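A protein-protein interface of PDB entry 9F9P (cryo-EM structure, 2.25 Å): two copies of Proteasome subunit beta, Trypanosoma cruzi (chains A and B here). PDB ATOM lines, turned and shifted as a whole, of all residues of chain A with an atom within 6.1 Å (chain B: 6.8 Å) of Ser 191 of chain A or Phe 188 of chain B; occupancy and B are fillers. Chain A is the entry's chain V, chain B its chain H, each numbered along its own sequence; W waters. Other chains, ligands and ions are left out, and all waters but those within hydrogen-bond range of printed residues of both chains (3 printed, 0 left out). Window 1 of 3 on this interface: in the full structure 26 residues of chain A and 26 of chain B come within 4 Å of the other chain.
Ile 187 of chain A touches Phe 188 of chain B, and with the chains exchanged Phe 188 of chain A touches Ile 187 of chain B. Phe 188 of chain A touches Ser 191 of chain B, and with the chains exchanged Ser 191 of chain A touches Phe 188 of chain B.
Among the printed residues, pairs that only touch across the chains: Tyr 190 of chain A with Arg 220 of chain B, Ile 187 of chain A with Phe 188 of chain B, Phe 188 of chain A with Ile 187 of chain B and Ala 195 of chain A with His 216 of chain B.
Water W1 lies within hydrogen-bond range of the backbone carbonyl oxygen (O) of Ile 187 of chain B (2.7 Å), the backbone NH (N) of Ser 191 of chain B (3.0 Å), the backbone carbonyl oxygen (O) of Phe 188 of chain A (3.4 Å) and the backbone NH (N) of Tyr 190 of chain B (3.4 Å). Water W3 lies within hydrogen-bond range of the backbone carbonyl oxygen of Ile 187 of chain A (2.7 Å), the backbone NH of Ser 191 of chain A (3.0 Å), the backbone carbonyl oxygen of Phe 188 of chain B (3.4 Å) and the backbone NH of Tyr 190 of chain A (3.4 Å). Water W2 lies within hydrogen-bond range of OD2 of Asp 194 of chain A (2.8 Å), ND1 of His 216 of chain B (2.9 Å) and OG of Ser 191 of chain A (3.3 Å).
Printed residues of chain B within 4 Å of Tyr 190 of chain A: Arg 220 (3.6 Å). Printed residues of chain B within 4 Å of Asp 194 of chain A: Arg 220. Printed residues of chain A within 4 Å of Ile 187 of chain B: Phe 188 (3.8 Å). Phe 188 of chain B touches just these residues of chain A: Ile 187 (3.8 Å) and Ser 191 (3.2 Å). Printed residues of chain A within 4 Å of Arg 220 of chain B: Tyr 190 (3.6 Å) and Asp 194 (2.7 Å). The nearest printed residue of chain A that does not touch Arg 220 of chain B is Ser 191 of chain A (4.7 Å).
OG of Ser 191 of chain B sits at hydrogen-bond distance from O of Phe 188 of chain A, at 3.2 Å. The guanidinium group (NH2) of Arg 220 of chain B lies within salt-bridge range of the side-chain carboxylate (OD1) of Asp 194 of chain A, at 2.7 Å. OG of Ser 191 of chain A is in hydrogen-bond range of O of Phe 188 of chain B, at 3.2 Å.
Printed residues of chain A that touch a printed residue of chain B: Ile 187, Phe 188, Tyr 190, Ser 191, Asp 194 and Ala 195. Of the 18 printed residues of chain B, 5 touch a printed residue of chain A. Printed residues of chain B that touch a printed residue of chain A: Ile 187, Phe 188, Ser 191, His 216 and Arg 220. Hydrophobic or aromatic side chains of chain B that line the printed part of chain A: Ile 187, Phe 188 and His 216.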
ATOM      1  N   ILE A 187      16.480 -22.289   9.211  1.00  0.00           N
ATOM      2  CA  ILE A 187      17.875 -22.708   9.180  1.00  0.00           C
ATOM      3  C   ILE A 187      18.241 -23.413  10.487  1.00  0.00           C
ATOM      4  O   ILE A 187      18.941 -24.408  10.452  1.00  0.00           O
ATOM      5  CB  ILE A 187      18.785 -21.515   8.823  1.00  0.00           C
ATOM      6  CG1 ILE A 187      20.142 -21.976   8.291  1.00  0.00           C
ATOM      7  CG2 ILE A 187      18.937 -20.529   9.972  1.00  0.00           C
ATOM      8  CD1 ILE A 187      20.151 -22.126   6.783  1.00  0.00           C
ATOM      9  N   PHE A 188      17.615 -23.021  11.605  1.00  0.00           N
ATOM     10  CA  PHE A 188      17.803 -23.635  12.903  1.00  0.00           C
ATOM     11  C   PHE A 188      17.148 -25.007  13.047  1.00  0.00           C
ATOM     12  O   PHE A 188      17.355 -25.666  14.075  1.00  0.00           O
ATOM     13  CB  PHE A 188      17.219 -22.722  13.998  1.00  0.00           C
ATOM     14  CG  PHE A 188      17.912 -21.386  14.084  1.00  0.00           C
ATOM     15  CD1 PHE A 188      19.193 -21.283  14.622  1.00  0.00           C
ATOM     16  CD2 PHE A 188      17.350 -20.248  13.538  1.00  0.00           C
ATOM     17  CE1 PHE A 188      19.873 -20.062  14.622  1.00  0.00           C
ATOM     18  CE2 PHE A 188      18.024 -19.027  13.540  1.00  0.00           C
ATOM     19  CZ  PHE A 188      19.293 -18.929  14.073  1.00  0.00           C
ATOM     20  N   LEU A 189      16.331 -25.439  12.076  1.00  0.00           N
ATOM     21  CA  LEU A 189      15.559 -26.652  12.246  1.00  0.00           C
ATOM     22  C   LEU A 189      15.967 -27.812  11.344  1.00  0.00           C
ATOM     23  O   LEU A 189      15.572 -28.934  11.625  1.00  0.00           O
ATOM     24  CB  LEU A 189      14.097 -26.292  11.987  1.00  0.00           C
ATOM     25  CG  LEU A 189      13.427 -25.466  13.073  1.00  0.00           C
ATOM     26  CD1 LEU A 189      11.930 -25.402  12.867  1.00  0.00           C
ATOM     27  CD2 LEU A 189      13.754 -26.041  14.442  1.00  0.00           C
ATOM     28  N   TYR A 190      16.713 -27.576  10.264  1.00  0.00           N
ATOM     29  CA  TYR A 190      17.199 -28.684   9.442  1.00  0.00           C
ATOM     30  C   TYR A 190      17.801 -29.783  10.300  1.00  0.00           C
ATOM     31  O   TYR A 190      17.391 -30.929  10.164  1.00  0.00           O
ATOM     32  CB  TYR A 190      18.140 -28.231   8.326  1.00  0.00           C
ATOM     33  CG  TYR A 190      17.372 -27.549   7.229  1.00  0.00           C
ATOM     34  CD1 TYR A 190      16.460 -28.272   6.486  1.00  0.00           C
ATOM     35  CD2 TYR A 190      17.440 -26.163   7.028  1.00  0.00           C
ATOM     36  CE1 TYR A 190      15.688 -27.659   5.514  1.00  0.00           C
ATOM     37  CE2 TYR A 190      16.654 -25.527   6.067  1.00  0.00           C
ATOM     38  CZ  TYR A 190      15.764 -26.285   5.313  1.00  0.00           C
ATOM     39  OH  TYR A 190      14.944 -25.742   4.327  1.00  0.00           O
ATOM     40  N   SER A 191      18.690 -29.457  11.225  1.00  0.00           N
ATOM     41  CA  SER A 191      19.324 -30.470  12.063  1.00  0.00           C
ATOM     42  C   SER A 191      18.382 -31.112  13.078  1.00  0.00           C
ATOM     43  O   SER A 191      18.544 -32.289  13.370  1.00  0.00           O
ATOM     44  CB  SER A 191      20.534 -29.893  12.751  1.00  0.00           C
ATOM     45  OG  SER A 191      21.588 -29.781  11.783  1.00  0.00           O
ATOM     46  N   PHE A 192      17.424 -30.356  13.616  1.00  0.00           N
ATOM     47  CA  PHE A 192      16.437 -30.882  14.552  1.00  0.00           C
ATOM     48  C   PHE A 192      15.595 -31.995  13.911  1.00  0.00           C
ATOM     49  O   PHE A 192      15.278 -32.981  14.538  1.00  0.00           O
ATOM     50  CB  PHE A 192      15.532 -29.726  15.017  1.00  0.00           C
ATOM     51  CG  PHE A 192      14.514 -30.071  16.071  1.00  0.00           C
ATOM     52  CD1 PHE A 192      14.867 -30.109  17.413  1.00  0.00           C
ATOM     53  CD2 PHE A 192      13.210 -30.375  15.729  1.00  0.00           C
ATOM     54  CE1 PHE A 192      13.938 -30.465  18.383  1.00  0.00           C
ATOM     55  CE2 PHE A 192      12.295 -30.789  16.692  1.00  0.00           C
ATOM     56  CZ  PHE A 192      12.660 -30.835  18.027  1.00  0.00           C
ATOM     57  N   PHE A 193      15.167 -31.803  12.662  1.00  0.00           N
ATOM     58  CA  PHE A 193      14.436 -32.813  11.912  1.00  0.00           C
ATOM     59  C   PHE A 193      15.318 -33.975  11.470  1.00  0.00           C
ATOM     60  O   PHE A 193      14.891 -35.108  11.499  1.00  0.00           O
ATOM     61  CB  PHE A 193      13.845 -32.210  10.634  1.00  0.00           C
ATOM     62  CG  PHE A 193      12.489 -31.594  10.803  1.00  0.00           C
ATOM     63  CD1 PHE A 193      12.331 -30.434  11.539  1.00  0.00           C
ATOM     64  CD2 PHE A 193      11.366 -32.210  10.279  1.00  0.00           C
ATOM     65  CE1 PHE A 193      11.078 -29.855  11.712  1.00  0.00           C
ATOM     66  CE2 PHE A 193      10.108 -31.673  10.514  1.00  0.00           C
ATOM     67  CZ  PHE A 193       9.960 -30.482  11.215  1.00  0.00           C
ATOM     68  N   ASP A 194      16.529 -33.701  10.989  1.00  0.00           N
ATOM     69  CA  ASP A 194      17.462 -34.761  10.624  1.00  0.00           C
ATOM     70  C   ASP A 194      17.696 -35.723  11.784  1.00  0.00           C
ATOM     71  O   ASP A 194      17.713 -36.925  11.575  1.00  0.00           O
ATOM     72  CB  ASP A 194      18.795 -34.197  10.102  1.00  0.00           C
ATOM     73  CG  ASP A 194      18.800 -33.636   8.683  1.00  0.00           C
ATOM     74  OD1 ASP A 194      17.803 -33.791   7.958  1.00  0.00           O
ATOM     75  OD2 ASP A 194      19.818 -33.019   8.302  1.00  0.00           O
ATOM     76  N   ALA A 195      17.815 -35.227  13.005  1.00  0.00           N
ATOM     77  CA  ALA A 195      17.973 -36.066  14.190  1.00  0.00           C
ATOM     78  C   ALA A 195      16.680 -36.661  14.776  1.00  0.00           C
ATOM     79  O   ALA A 195      16.760 -37.777  15.271  1.00  0.00           O
ATOM     80  CB  ALA A 195      18.691 -35.267  15.247  1.00  0.00           C
ATOM     81  N   ASN A 196      15.507 -35.986  14.768  1.00  0.00           N
ATOM     82  CA  ASN A 196      14.352 -36.400  15.592  1.00  0.00           C
ATOM     83  C   ASN A 196      13.026 -36.643  14.851  1.00  0.00           C
ATOM     84  O   ASN A 196      12.029 -36.883  15.527  1.00  0.00           O
ATOM     85  CB  ASN A 196      13.951 -35.328  16.612  1.00  0.00           C
ATOM     86  CG  ASN A 196      15.130 -34.704  17.338  1.00  0.00           C
ATOM     87  OD1 ASN A 196      15.211 -33.489  17.528  1.00  0.00           O
ATOM     88  ND2 ASN A 196      16.062 -35.543  17.752  1.00  0.00           N
ATOM     89  N   THR B  56      33.171 -25.857  10.187  1.00  0.00           N
ATOM     90  CA  THR B  56      32.491 -26.127  11.432  1.00  0.00           C
ATOM     91  C   THR B  56      33.515 -26.449  12.520  1.00  0.00           C
ATOM     92  O   THR B  56      34.218 -27.438  12.411  1.00  0.00           O
ATOM     93  CB  THR B  56      31.591 -27.359  11.260  1.00  0.00           C
ATOM     94  OG1 THR B  56      30.701 -27.263  10.132  1.00  0.00           O
ATOM     95  CG2 THR B  56      30.791 -27.604  12.512  1.00  0.00           C
ATOM     96  N   SER B 184      30.755 -21.204   9.454  1.00  0.00           N
ATOM     97  CA  SER B 184      29.526 -21.235   8.663  1.00  0.00           C
ATOM     98  C   SER B 184      28.562 -22.305   9.171  1.00  0.00           C
ATOM     99  O   SER B 184      27.374 -22.041   9.225  1.00  0.00           O
ATOM    100  CB  SER B 184      29.821 -21.443   7.190  1.00  0.00           C
ATOM    101  OG  SER B 184      30.309 -22.769   6.938  1.00  0.00           O
ATOM    102  N   GLY B 185      29.086 -23.447   9.626  1.00  0.00           N
ATOM    103  CA  GLY B 185      28.268 -24.573  10.050  1.00  0.00           C
ATOM    104  C   GLY B 185      27.666 -24.422  11.458  1.00  0.00           C
ATOM    105  O   GLY B 185      26.761 -25.145  11.833  1.00  0.00           O
ATOM    106  N   SER B 186      28.169 -23.508  12.267  1.00  0.00           N
ATOM    107  CA  SER B 186      27.643 -23.342  13.609  1.00  0.00           C
ATOM    108  C   SER B 186      26.131 -23.119  13.639  1.00  0.00           C
ATOM    109  O   SER B 186      25.505 -23.475  14.615  1.00  0.00           O
ATOM    110  CB  SER B 186      28.351 -22.200  14.344  1.00  0.00           C
ATOM    111  OG  SER B 186      28.300 -20.964  13.644  1.00  0.00           O
ATOM    112  N   ILE B 187      25.571 -22.420  12.642  1.00  0.00           N
ATOM    113  CA  ILE B 187      24.177 -22.004  12.677  1.00  0.00           C
ATOM    114  C   ILE B 187      23.264 -23.230  12.743  1.00  0.00           C
ATOM    115  O   ILE B 187      22.290 -23.209  13.470  1.00  0.00           O
ATOM    116  CB  ILE B 187      23.875 -21.047  11.506  1.00  0.00           C
ATOM    117  CG1 ILE B 187      22.624 -20.207  11.766  1.00  0.00           C
ATOM    118  CG2 ILE B 187      23.798 -21.766  10.166  1.00  0.00           C
ATOM    119  CD1 ILE B 187      22.944 -18.891  12.444  1.00  0.00           C
ATOM    120  N   PHE B 188      23.684 -24.354  12.145  1.00  0.00           N
ATOM    121  CA  PHE B 188      22.966 -25.613  12.177  1.00  0.00           C
ATOM    122  C   PHE B 188      23.029 -26.332  13.523  1.00  0.00           C
ATOM    123  O   PHE B 188      22.343 -27.350  13.692  1.00  0.00           O
ATOM    124  CB  PHE B 188      23.539 -26.565  11.110  1.00  0.00           C
ATOM    125  CG  PHE B 188      23.371 -26.044   9.705  1.00  0.00           C
ATOM    126  CD1 PHE B 188      22.120 -26.043   9.093  1.00  0.00           C
ATOM    127  CD2 PHE B 188      24.421 -25.457   9.025  1.00  0.00           C
ATOM    128  CE1 PHE B 188      21.944 -25.482   7.826  1.00  0.00           C
ATOM    129  CE2 PHE B 188      24.249 -24.900   7.758  1.00  0.00           C
ATOM    130  CZ  PHE B 188      23.008 -24.900   7.154  1.00  0.00           C
ATOM    131  N   LEU B 189      23.856 -25.866  14.468  1.00  0.00           N
ATOM    132  CA  LEU B 189      24.075 -26.611  15.691  1.00  0.00           C
ATOM    133  C   LEU B 189      23.523 -25.958  16.954  1.00  0.00           C
ATOM    134  O   LEU B 189      23.407 -26.644  17.959  1.00  0.00           O
ATOM    135  CB  LEU B 189      25.583 -26.805  15.833  1.00  0.00           C
ATOM    136  CG  LEU B 189      26.205 -27.803  14.869  1.00  0.00           C
ATOM    137  CD1 LEU B 189      27.625 -28.134  15.267  1.00  0.00           C
ATOM    138  CD2 LEU B 189      25.359 -29.064  14.806  1.00  0.00           C
ATOM    139  N   TYR B 190      23.210 -24.662  16.945  1.00  0.00           N
ATOM    140  CA  TYR B 190      22.587 -24.040  18.113  1.00  0.00           C
ATOM    141  C   TYR B 190      21.435 -24.884  18.635  1.00  0.00           C
ATOM    142  O   TYR B 190      21.429 -25.206  19.817  1.00  0.00           O
ATOM    143  CB  TYR B 190      22.185 -22.587  17.872  1.00  0.00           C
ATOM    144  CG  TYR B 190      23.396 -21.697  17.852  1.00  0.00           C
ATOM    145  CD1 TYR B 190      24.149 -21.546  19.000  1.00  0.00           C
ATOM    146  CD2 TYR B 190      23.878 -21.133  16.663  1.00  0.00           C
ATOM    147  CE1 TYR B 190      25.307 -20.787  18.995  1.00  0.00           C
ATOM    148  CE2 TYR B 190      25.055 -20.383  16.639  1.00  0.00           C
ATOM    149  CZ  TYR B 190      25.777 -20.222  17.816  1.00  0.00           C
ATOM    150  OH  TYR B 190      26.956 -19.486  17.887  1.00  0.00           O
ATOM    151  N   SER B 191      20.517 -25.309  17.783  1.00  0.00           N
ATOM    152  CA  SER B 191      19.374 -26.100  18.228  1.00  0.00           C
ATOM    153  C   SER B 191      19.734 -27.514  18.674  1.00  0.00           C
ATOM    154  O   SER B 191      19.095 -28.027  19.581  1.00  0.00           O
ATOM    155  CB  SER B 191      18.316 -26.134  17.154  1.00  0.00           C
ATOM    156  OG  SER B 191      17.656 -24.861  17.135  1.00  0.00           O
ATOM    157  N   PHE B 192      20.731 -28.140  18.045  1.00  0.00           N
ATOM    158  CA  PHE B 192      21.191 -29.470  18.427  1.00  0.00           C
ATOM    159  C   PHE B 192      21.713 -29.486  19.872  1.00  0.00           C
ATOM    160  O   PHE B 192      21.488 -30.420  20.608  1.00  0.00           O
ATOM    161  CB  PHE B 192      22.298 -29.908  17.452  1.00  0.00           C
ATOM    162  CG  PHE B 192      22.823 -31.307  17.638  1.00  0.00           C
ATOM    163  CD1 PHE B 192      22.152 -32.395  17.097  1.00  0.00           C
ATOM    164  CD2 PHE B 192      23.974 -31.544  18.366  1.00  0.00           C
ATOM    165  CE1 PHE B 192      22.614 -33.689  17.300  1.00  0.00           C
ATOM    166  CE2 PHE B 192      24.405 -32.843  18.620  1.00  0.00           C
ATOM    167  CZ  PHE B 192      23.722 -33.922  18.085  1.00  0.00           C
ATOM    168  N   PHE B 193      22.484 -28.470  20.260  1.00  0.00           N
ATOM    169  CA  PHE B 193      22.971 -28.321  21.623  1.00  0.00           C
ATOM    170  C   PHE B 193      21.877 -27.912  22.601  1.00  0.00           C
ATOM    171  O   PHE B 193      21.850 -28.386  23.716  1.00  0.00           O
ATOM    172  CB  PHE B 193      24.043 -27.227  21.695  1.00  0.00           C
ATOM    173  CG  PHE B 193      25.438 -27.701  21.426  1.00  0.00           C
ATOM    174  CD1 PHE B 193      25.808 -28.115  20.159  1.00  0.00           C
ATOM    175  CD2 PHE B 193      26.361 -27.792  22.453  1.00  0.00           C
ATOM    176  CE1 PHE B 193      27.097 -28.565  19.895  1.00  0.00           C
ATOM    177  CE2 PHE B 193      27.624 -28.312  22.205  1.00  0.00           C
ATOM    178  CZ  PHE B 193      28.004 -28.682  20.920  1.00  0.00           C
ATOM    179  N   ALA B 213      27.748 -34.053  16.434  1.00  0.00           N
ATOM    180  CA  ALA B 213      27.482 -32.661  16.132  1.00  0.00           C
ATOM    181  C   ALA B 213      28.177 -32.215  14.863  1.00  0.00           C
ATOM    182  O   ALA B 213      27.540 -31.585  14.037  1.00  0.00           O
ATOM    183  CB  ALA B 213      27.904 -31.818  17.287  1.00  0.00           C
ATOM    184  N   HIS B 216      26.284 -33.791  11.742  1.00  0.00           N
ATOM    185  CA  HIS B 216      25.065 -33.059  11.416  1.00  0.00           C
ATOM    186  C   HIS B 216      25.331 -31.741  10.721  1.00  0.00           C
ATOM    187  O   HIS B 216      24.657 -31.403   9.758  1.00  0.00           O
ATOM    188  CB  HIS B 216      24.175 -32.809  12.637  1.00  0.00           C
ATOM    189  CG  HIS B 216      23.417 -34.033  12.957  1.00  0.00           C
ATOM    190  ND1 HIS B 216      22.270 -34.398  12.278  1.00  0.00           N
ATOM    191  CD2 HIS B 216      23.628 -35.010  13.875  1.00  0.00           C
ATOM    192  CE1 HIS B 216      21.801 -35.552  12.783  1.00  0.00           C
ATOM    193  NE2 HIS B 216      22.622 -35.958  13.741  1.00  0.00           N
ATOM    194  N   ALA B 217      26.292 -30.969  11.176  1.00  0.00           N
ATOM    195  CA  ALA B 217      26.494 -29.699  10.518  1.00  0.00           C
ATOM    196  C   ALA B 217      27.022 -29.950   9.115  1.00  0.00           C
ATOM    197  O   ALA B 217      26.546 -29.321   8.168  1.00  0.00           O
ATOM    198  CB  ALA B 217      27.393 -28.789  11.336  1.00  0.00           C
ATOM    199  N   TYR B 218      27.947 -30.884   8.929  1.00  0.00           N
ATOM    200  CA  TYR B 218      28.493 -30.932   7.592  1.00  0.00           C
ATOM    201  C   TYR B 218      27.560 -31.601   6.577  1.00  0.00           C
ATOM    202  O   TYR B 218      27.737 -31.334   5.383  1.00  0.00           O
ATOM    203  CB  TYR B 218      29.958 -31.391   7.520  1.00  0.00           C
ATOM    204  CG  TYR B 218      30.355 -32.825   7.705  1.00  0.00           C
ATOM    205  CD1 TYR B 218      29.518 -33.880   7.445  1.00  0.00           C
ATOM    206  CD2 TYR B 218      31.657 -33.118   8.049  1.00  0.00           C
ATOM    207  CE1 TYR B 218      29.944 -35.194   7.604  1.00  0.00           C
ATOM    208  CE2 TYR B 218      32.108 -34.428   8.178  1.00  0.00           C
ATOM    209  CZ  TYR B 218      31.228 -35.471   8.010  1.00  0.00           C
ATOM    210  OH  TYR B 218      31.636 -36.766   8.153  1.00  0.00           O
ATOM    211  N   ARG B 220      24.512 -30.675   6.137  1.00  0.00           N
ATOM    212  CA  ARG B 220      23.663 -29.619   5.615  1.00  0.00           C
ATOM    213  C   ARG B 220      24.426 -28.439   5.030  1.00  0.00           C
ATOM    214  O   ARG B 220      23.803 -27.676   4.317  1.00  0.00           O
ATOM    215  CB  ARG B 220      22.709 -29.135   6.723  1.00  0.00           C
ATOM    216  CG  ARG B 220      21.618 -30.142   7.077  1.00  0.00           C
ATOM    217  CD  ARG B 220      20.615 -30.245   5.936  1.00  0.00           C
ATOM    218  NE  ARG B 220      19.532 -31.156   6.216  1.00  0.00           N
ATOM    219  CZ  ARG B 220      18.433 -31.293   5.477  1.00  0.00           C
ATOM    220  NH1 ARG B 220      18.243 -30.587   4.372  1.00  0.00           N
ATOM    221  NH2 ARG B 220      17.535 -32.175   5.854  1.00  0.00           N
ATOM    222  N   ASP B 221      25.690 -28.215   5.417  1.00  0.00           N
ATOM    223  CA  ASP B 221      26.474 -27.049   5.005  1.00  0.00           C
ATOM    224  C   ASP B 221      27.415 -27.441   3.869  1.00  0.00           C
ATOM    225  O   ASP B 221      28.301 -28.294   4.052  1.00  0.00           O
ATOM    226  CB  ASP B 221      27.289 -26.488   6.173  1.00  0.00           C
ATOM    227  CG  ASP B 221      28.146 -25.249   5.893  1.00  0.00           C
ATOM    228  OD1 ASP B 221      27.900 -24.540   4.877  1.00  0.00           O
ATOM    229  OD2 ASP B 221      29.105 -24.982   6.698  1.00  0.00           O
ATOM    230  N   GLY B 222      27.232 -26.824   2.694  1.00  0.00           N
ATOM    231  CA  GLY B 222      28.078 -27.093   1.528  1.00  0.00           C
ATOM    232  C   GLY B 222      29.545 -26.683   1.713  1.00  0.00           C
ATOM    233  O   GLY B 222      30.429 -27.292   1.129  1.00  0.00           O
HETATM  234  O   HOH W   1      20.447 -24.564  14.923  1.00  0.00           O
HETATM  235  O   HOH W   2      21.936 -32.610  10.075  1.00  0.00           O
HETATM  236  O   HOH W   3      19.743 -26.724  11.616  1.00  0.00           O
